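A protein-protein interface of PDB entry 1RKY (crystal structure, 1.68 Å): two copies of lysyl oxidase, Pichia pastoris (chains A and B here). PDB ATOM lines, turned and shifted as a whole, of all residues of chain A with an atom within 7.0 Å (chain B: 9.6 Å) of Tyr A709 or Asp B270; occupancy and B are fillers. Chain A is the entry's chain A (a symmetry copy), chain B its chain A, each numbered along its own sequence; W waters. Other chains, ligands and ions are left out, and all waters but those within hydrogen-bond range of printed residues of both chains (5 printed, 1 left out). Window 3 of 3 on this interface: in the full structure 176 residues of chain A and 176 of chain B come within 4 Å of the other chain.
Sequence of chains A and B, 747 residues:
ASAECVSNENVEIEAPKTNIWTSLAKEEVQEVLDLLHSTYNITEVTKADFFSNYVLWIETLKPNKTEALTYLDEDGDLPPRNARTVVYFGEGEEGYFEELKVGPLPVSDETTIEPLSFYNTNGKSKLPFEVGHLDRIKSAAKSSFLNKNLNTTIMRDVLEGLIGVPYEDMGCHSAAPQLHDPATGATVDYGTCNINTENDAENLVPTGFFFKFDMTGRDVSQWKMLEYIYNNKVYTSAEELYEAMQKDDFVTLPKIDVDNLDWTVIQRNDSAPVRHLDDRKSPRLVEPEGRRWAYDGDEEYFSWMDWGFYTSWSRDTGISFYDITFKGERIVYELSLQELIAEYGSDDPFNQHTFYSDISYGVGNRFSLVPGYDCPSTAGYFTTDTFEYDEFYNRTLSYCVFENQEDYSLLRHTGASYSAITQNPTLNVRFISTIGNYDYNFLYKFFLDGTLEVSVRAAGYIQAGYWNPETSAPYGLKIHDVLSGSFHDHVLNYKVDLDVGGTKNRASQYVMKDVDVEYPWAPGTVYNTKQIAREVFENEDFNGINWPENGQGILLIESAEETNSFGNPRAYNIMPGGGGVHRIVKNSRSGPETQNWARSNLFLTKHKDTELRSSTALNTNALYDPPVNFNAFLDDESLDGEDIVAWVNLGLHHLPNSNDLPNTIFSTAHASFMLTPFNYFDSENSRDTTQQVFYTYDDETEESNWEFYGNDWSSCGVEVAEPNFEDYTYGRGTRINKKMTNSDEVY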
ATOM      1  N   ILE A 421      28.629  -2.754 -12.151  1.00  0.00           N
ATOM      2  CA  ILE A 421      28.668  -3.836 -11.155  1.00  0.00           C
ATOM      3  C   ILE A 421      28.499  -5.214 -11.816  1.00  0.00           C
ATOM      4  O   ILE A 421      27.660  -5.402 -12.703  1.00  0.00           O
ATOM      5  CB  ILE A 421      27.572  -3.619 -10.078  1.00  0.00           C
ATOM      6  CG1 ILE A 421      27.576  -2.211  -9.540  1.00  0.00           C
ATOM      7  CG2 ILE A 421      27.747  -4.620  -8.866  1.00  0.00           C
ATOM      8  CD1 ILE A 421      26.405  -1.886  -8.713  1.00  0.00           C
ATOM      9  N   THR A 689      30.962 -11.858 -18.891  1.00  0.00           N
ATOM     10  CA  THR A 689      29.677 -12.286 -18.387  1.00  0.00           C
ATOM     11  C   THR A 689      28.575 -11.281 -18.689  1.00  0.00           C
ATOM     12  O   THR A 689      28.794 -10.082 -18.699  1.00  0.00           O
ATOM     13  CB  THR A 689      29.718 -12.602 -16.864  1.00  0.00           C
ATOM     14  OG1 THR A 689      28.441 -13.137 -16.480  1.00  0.00           O
ATOM     15  CG2 THR A 689      29.871 -11.357 -16.050  1.00  0.00           C
ATOM     16  N   THR A 690      27.373 -11.794 -18.921  1.00  0.00           N
ATOM     17  CA  THR A 690      26.201 -10.946 -19.031  1.00  0.00           C
ATOM     18  C   THR A 690      25.627 -10.564 -17.684  1.00  0.00           C
ATOM     19  O   THR A 690      24.721  -9.751 -17.637  1.00  0.00           O
ATOM     20  CB  THR A 690      25.081 -11.636 -19.810  1.00  0.00           C
ATOM     21  OG1 THR A 690      24.637 -12.808 -19.079  1.00  0.00           O
ATOM     22  CG2 THR A 690      25.578 -12.139 -21.161  1.00  0.00           C
ATOM     23  N   GLN A 691      26.113 -11.157 -16.575  1.00  0.00           N
ATOM     24  CA  GLN A 691      25.505 -10.907 -15.283  1.00  0.00           C
ATOM     25  C   GLN A 691      26.093  -9.688 -14.637  1.00  0.00           C
ATOM     26  O   GLN A 691      26.801  -9.758 -13.637  1.00  0.00           O
ATOM     27  CB  GLN A 691      25.630 -12.168 -14.396  1.00  0.00           C
ATOM     28  CG  GLN A 691      25.036 -13.395 -15.010  1.00  0.00           C
ATOM     29  CD  GLN A 691      23.555 -13.257 -15.282  1.00  0.00           C
ATOM     30  OE1 GLN A 691      22.773 -13.091 -14.355  1.00  0.00           O
ATOM     31  NE2 GLN A 691      23.163 -13.310 -16.564  1.00  0.00           N
ATOM     32  N   GLN A 692      25.834  -8.549 -15.255  1.00  0.00           N
ATOM     33  CA  GLN A 692      26.393  -7.285 -14.819  1.00  0.00           C
ATOM     34  C   GLN A 692      25.457  -6.175 -15.265  1.00  0.00           C
ATOM     35  O   GLN A 692      24.536  -6.406 -16.076  1.00  0.00           O
ATOM     36  CB  GLN A 692      27.839  -7.070 -15.335  1.00  0.00           C
ATOM     37  CG  GLN A 692      28.056  -7.208 -16.818  1.00  0.00           C
ATOM     38  CD  GLN A 692      29.488  -6.869 -17.194  1.00  0.00           C
ATOM     39  OE1 GLN A 692      29.895  -5.721 -17.095  1.00  0.00           O
ATOM     40  NE2 GLN A 692      30.254  -7.858 -17.623  1.00  0.00           N
ATOM     41  N   VAL A 693      25.654  -5.003 -14.676  1.00  0.00           N
ATOM     42  CA  VAL A 693      24.909  -3.799 -14.999  1.00  0.00           C
ATOM     43  C   VAL A 693      25.874  -2.668 -15.335  1.00  0.00           C
ATOM     44  O   VAL A 693      26.978  -2.558 -14.796  1.00  0.00           O
ATOM     45  CB  VAL A 693      23.928  -3.386 -13.863  1.00  0.00           C
ATOM     46  CG1 VAL A 693      24.678  -3.035 -12.557  1.00  0.00           C
ATOM     47  CG2 VAL A 693      23.065  -2.202 -14.269  1.00  0.00           C
ATOM     48  N   PHE A 694      25.474  -1.831 -16.288  1.00  0.00           N
ATOM     49  CA  PHE A 694      26.215  -0.624 -16.613  1.00  0.00           C
ATOM     50  C   PHE A 694      25.220   0.522 -16.594  1.00  0.00           C
ATOM     51  O   PHE A 694      24.365   0.624 -17.463  1.00  0.00           O
ATOM     52  CB  PHE A 694      26.908  -0.730 -17.967  1.00  0.00           C
ATOM     53  CG  PHE A 694      27.775   0.453 -18.304  1.00  0.00           C
ATOM     54  CD1 PHE A 694      27.616   1.117 -19.513  1.00  0.00           C
ATOM     55  CD2 PHE A 694      28.759   0.901 -17.431  1.00  0.00           C
ATOM     56  CE1 PHE A 694      28.402   2.209 -19.826  1.00  0.00           C
ATOM     57  CE2 PHE A 694      29.556   1.992 -17.755  1.00  0.00           C
ATOM     58  CZ  PHE A 694      29.372   2.647 -18.948  1.00  0.00           C
ATOM     59  N   TRP A 706      20.119   2.425 -17.974  1.00  0.00           N
ATOM     60  CA  TRP A 706      20.472   1.137 -17.381  1.00  0.00           C
ATOM     61  C   TRP A 706      20.684   0.102 -18.471  1.00  0.00           C
ATOM     62  O   TRP A 706      19.781  -0.156 -19.265  1.00  0.00           O
ATOM     63  CB  TRP A 706      19.345   0.667 -16.482  1.00  0.00           C
ATOM     64  CG  TRP A 706      19.116   1.524 -15.295  1.00  0.00           C
ATOM     65  CD1 TRP A 706      18.347   2.657 -15.227  1.00  0.00           C
ATOM     66  CD2 TRP A 706      19.642   1.316 -13.977  1.00  0.00           C
ATOM     67  NE1 TRP A 706      18.357   3.161 -13.947  1.00  0.00           N
ATOM     68  CE2 TRP A 706      19.138   2.354 -13.156  1.00  0.00           C
ATOM     69  CE3 TRP A 706      20.461   0.334 -13.396  1.00  0.00           C
ATOM     70  CZ2 TRP A 706      19.455   2.460 -11.795  1.00  0.00           C
ATOM     71  CZ3 TRP A 706      20.777   0.442 -12.031  1.00  0.00           C
ATOM     72  CH2 TRP A 706      20.280   1.504 -11.257  1.00  0.00           C
ATOM     73  N   GLU A 707      21.874  -0.481 -18.517  1.00  0.00           N
ATOM     74  CA  GLU A 707      22.182  -1.569 -19.436  1.00  0.00           C
ATOM     75  C   GLU A 707      22.298  -2.860 -18.614  1.00  0.00           C
ATOM     76  O   GLU A 707      23.177  -2.962 -17.762  1.00  0.00           O
ATOM     77  CB  GLU A 707      23.480  -1.339 -20.158  1.00  0.00           C
ATOM     78  CG  GLU A 707      23.934  -2.522 -21.007  1.00  0.00           C
ATOM     79  CD  GLU A 707      22.947  -2.839 -22.122  1.00  0.00           C
ATOM     80  OE1 GLU A 707      22.773  -1.963 -22.998  1.00  0.00           O
ATOM     81  OE2 GLU A 707      22.339  -3.938 -22.122  1.00  0.00           O
ATOM     82  N   PHE A 708      21.465  -3.832 -18.930  1.00  0.00           N
ATOM     83  CA  PHE A 708      21.374  -5.090 -18.183  1.00  0.00           C
ATOM     84  C   PHE A 708      21.812  -6.294 -19.010  1.00  0.00           C
ATOM     85  O   PHE A 708      21.665  -7.445 -18.562  1.00  0.00           O
ATOM     86  CB  PHE A 708      19.947  -5.327 -17.718  1.00  0.00           C
ATOM     87  CG  PHE A 708      19.479  -4.382 -16.660  1.00  0.00           C
ATOM     88  CD1 PHE A 708      18.494  -3.451 -16.930  1.00  0.00           C
ATOM     89  CD2 PHE A 708      20.002  -4.445 -15.376  1.00  0.00           C
ATOM     90  CE1 PHE A 708      18.046  -2.593 -15.941  1.00  0.00           C
ATOM     91  CE2 PHE A 708      19.555  -3.602 -14.381  1.00  0.00           C
ATOM     92  CZ  PHE A 708      18.581  -2.665 -14.662  1.00  0.00           C
ATOM     93  N   TYR A 709      22.324  -6.049 -20.209  1.00  0.00           N
ATOM     94  CA  TYR A 709      22.890  -7.105 -21.063  1.00  0.00           C
ATOM     95  C   TYR A 709      21.985  -8.324 -21.270  1.00  0.00           C
ATOM     96  O   TYR A 709      22.441  -9.479 -21.250  1.00  0.00           O
ATOM     97  CB  TYR A 709      24.265  -7.518 -20.516  1.00  0.00           C
ATOM     98  CG  TYR A 709      25.219  -6.375 -20.467  1.00  0.00           C
ATOM     99  CD1 TYR A 709      25.523  -5.733 -19.275  1.00  0.00           C
ATOM    100  CD2 TYR A 709      25.811  -5.888 -21.636  1.00  0.00           C
ATOM    101  CE1 TYR A 709      26.390  -4.672 -19.254  1.00  0.00           C
ATOM    102  CE2 TYR A 709      26.666  -4.831 -21.616  1.00  0.00           C
ATOM    103  CZ  TYR A 709      26.974  -4.228 -20.414  1.00  0.00           C
ATOM    104  OH  TYR A 709      27.831  -3.159 -20.385  1.00  0.00           O
ATOM    105  N   GLY A 710      20.690  -8.069 -21.473  1.00  0.00           N
ATOM    106  CA  GLY A 710      19.757  -9.124 -21.824  1.00  0.00           C
ATOM    107  C   GLY A 710      19.025  -9.760 -20.667  1.00  0.00           C
ATOM    108  O   GLY A 710      18.170 -10.618 -20.861  1.00  0.00           O
ATOM    109  N   ASN A 711      19.358  -9.330 -19.450  1.00  0.00           N
ATOM    110  CA  ASN A 711      18.685  -9.778 -18.252  1.00  0.00           C
ATOM    111  C   ASN A 711      17.511  -8.891 -17.897  1.00  0.00           C
ATOM    112  O   ASN A 711      17.669  -7.698 -17.671  1.00  0.00           O
ATOM    113  CB  ASN A 711      19.672  -9.806 -17.086  1.00  0.00           C
ATOM    114  CG  ASN A 711      20.797 -10.785 -17.340  1.00  0.00           C
ATOM    115  OD1 ASN A 711      20.615 -12.005 -17.227  1.00  0.00           O
ATOM    116  ND2 ASN A 711      21.934 -10.263 -17.765  1.00  0.00           N
ATOM    117  N   ASP A 712      16.337  -9.495 -17.831  1.00  0.00           N
ATOM    118  CA  ASP A 712      15.111  -8.750 -17.588  1.00  0.00           C
ATOM    119  C   ASP A 712      14.799  -8.836 -16.109  1.00  0.00           C
ATOM    120  O   ASP A 712      14.459  -9.905 -15.605  1.00  0.00           O
ATOM    121  CB  ASP A 712      13.976  -9.351 -18.440  1.00  0.00           C
ATOM    122  CG  ASP A 712      12.706  -8.524 -18.408  1.00  0.00           C
ATOM    123  OD1 ASP A 712      12.631  -7.593 -17.583  1.00  0.00           O
ATOM    124  OD2 ASP A 712      11.736  -8.734 -19.173  1.00  0.00           O
ATOM    125  N   VAL B 265      38.633  -0.476 -19.675  1.00  0.00           N
ATOM    126  CA  VAL B 265      37.168  -0.408 -19.608  1.00  0.00           C
ATOM    127  C   VAL B 265      36.575  -1.593 -18.849  1.00  0.00           C
ATOM    128  O   VAL B 265      36.839  -2.755 -19.158  1.00  0.00           O
ATOM    129  CB  VAL B 265      36.525  -0.329 -21.055  1.00  0.00           C
ATOM    130  CG1 VAL B 265      35.029  -0.289 -20.996  1.00  0.00           C
ATOM    131  CG2 VAL B 265      37.050   0.865 -21.769  1.00  0.00           C
ATOM    132  N   ILE B 266      35.730  -1.290 -17.871  1.00  0.00           N
ATOM    133  CA  ILE B 266      35.176  -2.327 -16.988  1.00  0.00           C
ATOM    134  C   ILE B 266      34.042  -3.109 -17.606  1.00  0.00           C
ATOM    135  O   ILE B 266      34.021  -4.340 -17.553  1.00  0.00           O
ATOM    136  CB  ILE B 266      34.679  -1.671 -15.675  1.00  0.00           C
ATOM    137  CG1 ILE B 266      35.848  -1.059 -14.943  1.00  0.00           C
ATOM    138  CG2 ILE B 266      33.942  -2.686 -14.795  1.00  0.00           C
ATOM    139  CD1 ILE B 266      35.421  -0.084 -13.847  1.00  0.00           C
ATOM    140  N   GLN B 267      33.070  -2.391 -18.161  1.00  0.00           N
ATOM    141  CA  GLN B 267      31.819  -3.010 -18.540  1.00  0.00           C
ATOM    142  C   GLN B 267      32.005  -3.896 -19.770  1.00  0.00           C
ATOM    143  O   GLN B 267      32.995  -3.803 -20.514  1.00  0.00           O
ATOM    144  CB  GLN B 267      30.707  -1.978 -18.723  1.00  0.00           C
ATOM    145  CG  GLN B 267      30.795  -1.127 -20.014  1.00  0.00           C
ATOM    146  CD  GLN B 267      31.700   0.075 -19.882  1.00  0.00           C
ATOM    147  OE1 GLN B 267      32.372   0.250 -18.858  1.00  0.00           O
ATOM    148  NE2 GLN B 267      31.711   0.933 -20.915  1.00  0.00           N
ATOM    149  N   ARG B 268      31.040  -4.778 -19.929  1.00  0.00           N
ATOM    150  CA  ARG B 268      31.021  -5.759 -20.983  1.00  0.00           C
ATOM    151  C   ARG B 268      31.151  -5.103 -22.367  1.00  0.00           C
ATOM    152  O   ARG B 268      30.565  -4.080 -22.643  1.00  0.00           O
ATOM    153  CB  ARG B 268      29.713  -6.535 -20.921  1.00  0.00           C
ATOM    154  CG  ARG B 268      29.641  -7.683 -21.849  1.00  0.00           C
ATOM    155  CD  ARG B 268      28.392  -8.534 -21.705  1.00  0.00           C
ATOM    156  NE  ARG B 268      28.763  -9.849 -22.115  1.00  0.00           N
ATOM    157  CZ  ARG B 268      28.932 -10.222 -23.367  1.00  0.00           C
ATOM    158  NH1 ARG B 268      28.624  -9.430 -24.391  1.00  0.00           N
ATOM    159  NH2 ARG B 268      29.381 -11.429 -23.595  1.00  0.00           N
ATOM    160  N   ASN B 269      31.954  -5.739 -23.197  1.00  0.00           N
ATOM    161  CA  ASN B 269      32.073  -5.474 -24.629  1.00  0.00           C
ATOM    162  C   ASN B 269      30.927  -6.232 -25.316  1.00  0.00           C
ATOM    163  O   ASN B 269      30.960  -7.452 -25.389  1.00  0.00           O
ATOM    164  CB  ASN B 269      33.433  -6.010 -25.071  1.00  0.00           C
ATOM    165  CG  ASN B 269      33.851  -5.549 -26.450  1.00  0.00           C
ATOM    166  OD1 ASN B 269      33.025  -5.400 -27.346  1.00  0.00           O
ATOM    167  ND2 ASN B 269      35.167  -5.328 -26.613  1.00  0.00           N
ATOM    168  N   ASP B 270      29.907  -5.542 -25.817  1.00  0.00           N
ATOM    169  CA  ASP B 270      28.744  -6.267 -26.360  1.00  0.00           C
ATOM    170  C   ASP B 270      29.007  -7.034 -27.685  1.00  0.00           C
ATOM    171  O   ASP B 270      28.113  -7.724 -28.180  1.00  0.00           O
ATOM    172  CB  ASP B 270      27.499  -5.361 -26.454  1.00  0.00           C
ATOM    173  CG  ASP B 270      26.349  -5.840 -25.551  1.00  0.00           C
ATOM    174  OD1 ASP B 270      25.351  -5.094 -25.419  1.00  0.00           O
ATOM    175  OD2 ASP B 270      26.351  -6.941 -24.934  1.00  0.00           O
ATOM    176  N   SER B 271      30.239  -6.959 -28.205  1.00  0.00           N
ATOM    177  CA  SER B 271      30.705  -7.837 -29.293  1.00  0.00           C
ATOM    178  C   SER B 271      31.377  -9.144 -28.803  1.00  0.00           C
ATOM    179  O   SER B 271      31.715 -10.020 -29.604  1.00  0.00           O
ATOM    180  CB  SER B 271      31.661  -7.072 -30.225  1.00  0.00           C
ATOM    181  OG  SER B 271      33.012  -7.158 -29.794  1.00  0.00           O
ATOM    182  N   ALA B 272      31.594  -9.272 -27.500  1.00  0.00           N
ATOM    183  CA  ALA B 272      32.103 -10.510 -26.943  1.00  0.00           C
ATOM    184  C   ALA B 272      31.038 -11.627 -27.019  1.00  0.00           C
ATOM    185  O   ALA B 272      29.843 -11.388 -26.822  1.00  0.00           O
ATOM    186  CB  ALA B 272      32.547 -10.292 -25.499  1.00  0.00           C
ATOM    187  N   PRO B 273      31.467 -12.846 -27.310  1.00  0.00           N
ATOM    188  CA  PRO B 273      30.551 -13.987 -27.272  1.00  0.00           C
ATOM    189  C   PRO B 273      30.011 -14.168 -25.860  1.00  0.00           C
ATOM    190  O   PRO B 273      30.635 -13.743 -24.892  1.00  0.00           O
ATOM    191  CB  PRO B 273      31.420 -15.186 -27.674  1.00  0.00           C
ATOM    192  CG  PRO B 273      32.781 -14.669 -27.992  1.00  0.00           C
ATOM    193  CD  PRO B 273      32.833 -13.218 -27.709  1.00  0.00           C
ATOM    194  N   VAL B 274      28.857 -14.791 -25.755  1.00  0.00           N
ATOM    195  CA  VAL B 274      28.246 -15.053 -24.464  1.00  0.00           C
ATOM    196  C   VAL B 274      28.612 -16.477 -24.065  1.00  0.00           C
ATOM    197  O   VAL B 274      28.613 -17.390 -24.897  1.00  0.00           O
ATOM    198  CB  VAL B 274      26.708 -14.838 -24.569  1.00  0.00           C
ATOM    199  CG1 VAL B 274      25.926 -15.519 -23.466  1.00  0.00           C
ATOM    200  CG2 VAL B 274      26.407 -13.343 -24.591  1.00  0.00           C
ATOM    201  N   ASP B 278      24.649 -18.323 -20.269  1.00  0.00           N
ATOM    202  CA  ASP B 278      24.658 -16.977 -19.694  1.00  0.00           C
ATOM    203  C   ASP B 278      23.537 -16.103 -20.265  1.00  0.00           C
ATOM    204  O   ASP B 278      23.419 -14.951 -19.893  1.00  0.00           O
ATOM    205  CB  ASP B 278      26.019 -16.322 -19.898  1.00  0.00           C
ATOM    206  CG  ASP B 278      26.459 -15.446 -18.735  1.00  0.00           C
ATOM    207  OD1 ASP B 278      25.841 -15.442 -17.650  1.00  0.00           O
ATOM    208  OD2 ASP B 278      27.486 -14.729 -18.856  1.00  0.00           O
ATOM    209  N   ASP B 279      22.710 -16.667 -21.151  1.00  0.00           N
ATOM    210  CA  ASP B 279      21.469 -16.026 -21.562  1.00  0.00           C
ATOM    211  C   ASP B 279      20.313 -16.366 -20.629  1.00  0.00           C
ATOM    212  O   ASP B 279      19.183 -15.998 -20.916  1.00  0.00           O
ATOM    213  CB  ASP B 279      21.112 -16.345 -23.044  1.00  0.00           C
ATOM    214  CG  ASP B 279      21.035 -17.830 -23.359  1.00  0.00           C
ATOM    215  OD1 ASP B 279      21.501 -18.698 -22.573  1.00  0.00           O
ATOM    216  OD2 ASP B 279      20.521 -18.227 -24.437  1.00  0.00           O
ATOM    217  N   ARG B 280      20.593 -17.065 -19.517  1.00  0.00           N
ATOM    218  CA  ARG B 280      19.627 -17.297 -18.467  1.00  0.00           C
ATOM    219  C   ARG B 280      20.078 -16.426 -17.303  1.00  0.00           C
ATOM    220  O   ARG B 280      21.284 -16.334 -17.057  1.00  0.00           O
ATOM    221  CB  ARG B 280      19.597 -18.764 -18.028  1.00  0.00           C
ATOM    222  CG  ARG B 280      19.245 -19.752 -19.116  1.00  0.00           C
ATOM    223  CD  ARG B 280      19.269 -21.177 -18.665  1.00  0.00           C
ATOM    224  NE  ARG B 280      18.957 -22.028 -19.804  1.00  0.00           N
ATOM    225  CZ  ARG B 280      18.606 -23.287 -19.730  1.00  0.00           C
ATOM    226  NH1 ARG B 280      18.526 -23.893 -18.567  1.00  0.00           N
ATOM    227  NH2 ARG B 280      18.288 -23.942 -20.862  1.00  0.00           N
ATOM    228  N   LYS B 281      19.133 -15.782 -16.629  1.00  0.00           N
ATOM    229  CA  LYS B 281      19.406 -14.926 -15.447  1.00  0.00           C
ATOM    230  C   LYS B 281      19.982 -15.754 -14.294  1.00  0.00           C
ATOM    231  O   LYS B 281      19.504 -16.863 -14.016  1.00  0.00           O
ATOM    232  CB  LYS B 281      18.093 -14.313 -14.925  1.00  0.00           C
ATOM    233  CG  LYS B 281      17.608 -13.074 -15.645  1.00  0.00           C
ATOM    234  CD  LYS B 281      16.508 -12.344 -14.841  1.00  0.00           C
ATOM    235  CE  LYS B 281      15.104 -12.832 -15.219  1.00  0.00           C
ATOM    236  NZ  LYS B 281      14.022 -12.363 -14.289  1.00  0.00           N
ATOM    237  N   TYR B 373      22.154  -5.383  -7.120  1.00  0.00           N
ATOM    238  CA  TYR B 373      23.534  -5.730  -7.440  1.00  0.00           C
ATOM    239  C   TYR B 373      24.484  -5.568  -6.265  1.00  0.00           C
ATOM    240  O   TYR B 373      25.262  -6.477  -5.981  1.00  0.00           O
ATOM    241  CB  TYR B 373      24.024  -4.851  -8.565  1.00  0.00           C
ATOM    242  CG  TYR B 373      23.385  -5.239  -9.848  1.00  0.00           C
ATOM    243  CD1 TYR B 373      22.138  -4.732 -10.191  1.00  0.00           C
ATOM    244  CD2 TYR B 373      23.995  -6.158 -10.705  1.00  0.00           C
ATOM    245  CE1 TYR B 373      21.509  -5.111 -11.372  1.00  0.00           C
ATOM    246  CE2 TYR B 373      23.377  -6.549 -11.882  1.00  0.00           C
ATOM    247  CZ  TYR B 373      22.126  -6.024 -12.196  1.00  0.00           C
ATOM    248  OH  TYR B 373      21.517  -6.368 -13.358  1.00  0.00           O
HETATM  249  O   HOH W   1      11.596 -10.875 -15.563  1.00  0.00           O
HETATM  250  O   HOH W   2      27.452 -15.744 -15.478  1.00  0.00           O
HETATM  251  O   HOH W   3      28.193  -1.874 -22.584  1.00  0.00           O
HETATM  252  O   HOH W   4      17.954 -13.607 -19.748  1.00  0.00           O
HETATM  253  O   HOH W   5      22.189  -7.941 -15.319  1.00  0.00           O
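N of Gln A691 lies within hydrogen-bond range of OG1 of Thr A689, 3.1 Å away. The side-chain hydroxyl of Thr A690 is in hydrogen-bond range of the side-chain amide nitrogen of Gln A691, at 3.0 Å. O of Thr A689 is in hydrogen-bond range of NE2 of Gln A692. The backbone carbonyl oxygen (O) of Phe A708 lies within hydrogen-bond range of the side-chain amide nitrogen (ND2) of Asn A711. The guanidinium group (NH2) of Arg B268 sits at hydrogen-bond distance from the backbone carbonyl oxygen (O) of Pro B273 (2.9 Å). The backbone carbonyl oxygen (O) of Ile A421 is in hydrogen-bond range of the backbone NH (N) of Val A693 (2.8 Å).
Water W3 lies within hydrogen-bond range of OH of Tyr A709 (2.6 Å) and O of Arg B268 (3.2 Å). Water W5 lies within hydrogen-bond range of OH of Tyr B373 (2.6 Å), O of Gln A692 (2.9 Å), O of Phe A708 (3.3 Å) and ND2 of Asn A711 (3.4 Å). Water W2 bridges OD1 of Asp B278 (2.7 Å) and OG1 of Thr A689 (3.0 Å). Water W4 bridges O of Asp B279 (2.9 Å) and O of Gly A710 (3.2 Å). Water W1 lies within hydrogen-bond range of the backbone carbonyl oxygen (O) of Asp A712 (3.0 Å) and the side-chain amino group (NZ) of Lys B281 (3.1 Å).
Of chain B, only Gln B267 (3.5 Å), Arg B268 (3.6 Å) and Asp B270 (3.5 Å) come within 4 Å of Tyr A709. Asp B270 touches one residue of chain A. No residue of chain B comes within 4 Å of Gly A710. Of the printed residues of chain B, Thr A689 touches Arg B268 (3.4 Å) and Asp B278 (3.0 Å). Of the printed residues of chain A, Asp B278 touches Thr A689 (3.0 Å), Thr A690 (2.6 Å) and Gln A691 (3.4 Å). Ile B266 touches none of the printed residues of chain A. Val B265 touches none of the printed residues of chain A. The nearest residue of chain A that does not touch Asp B270 is Glu A707 (4.6 Å).
Of the 14 printed residues of chain A, 11 touch a printed residue of chain B. Hydrophobic or aromatic side chains of chain A within 4 Å of the printed part of chain B: Ile A421, Val A693, Phe A694, Phe A708 and Tyr A709. Hydrophobic or aromatic side chains of chain B that line the printed part of chain A: Val B274 and Tyr B373. Among the printed residues, no Asp or Glu carboxylate lies within 4 Å of a Lys or Arg side-chain nitrogen of the other chain.
Among the printed residues, merely in contact across the chains: Phe A708 with Tyr B373 (3.2 Å), Gln A691 with Asp B278 (3.4 Å), Phe A694 with Gln B267 (3.5 Å), Tyr A709 with Asp B270 (3.5 Å), Tyr A709 with Gln B267 (3.5 Å), Tyr A709 with Arg B268 (3.6 Å), Asn A711 with Lys B281 (3.6 Å), Gln A691 with Arg B280 (3.6 Å), Val A693 with Tyr B373 (3.6 Å), Gln A692 with Gln B267 (3.6 Å), Thr A690 with Val B274 (3.7 Å), Ile A421 with Tyr B373 (3.7 Å), Gln A691 with Lys B281 (3.9 Å), Gln A692 with Tyr B373 (3.99 Å) and Thr A690 with Arg B268 (3.99 Å).
No position is printed for both chains. Of the 20 pairs that touch across the chains among the printed residues, none has its exchanged pair printed and touching as well.
The side-chain amino group (NZ) of Lys B281 lies within hydrogen-bond range of the backbone carbonyl oxygen (O) of Asp A712 (2.8 Å). The side-chain carboxylate of Asp B278 sits at hydrogen-bond distance from the side-chain hydroxyl of Thr A689 (3.0 Å). OG1 of Thr A690 is in hydrogen-bond range of O of Asp B278, at 2.6 Å. The backbone NH (N) of Arg B268 is in hydrogen-bond range of the side-chain amide oxygen (OE1) of Gln A692, at 3.2 Å. NE of Arg B268 sits close to O of Thr A689.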
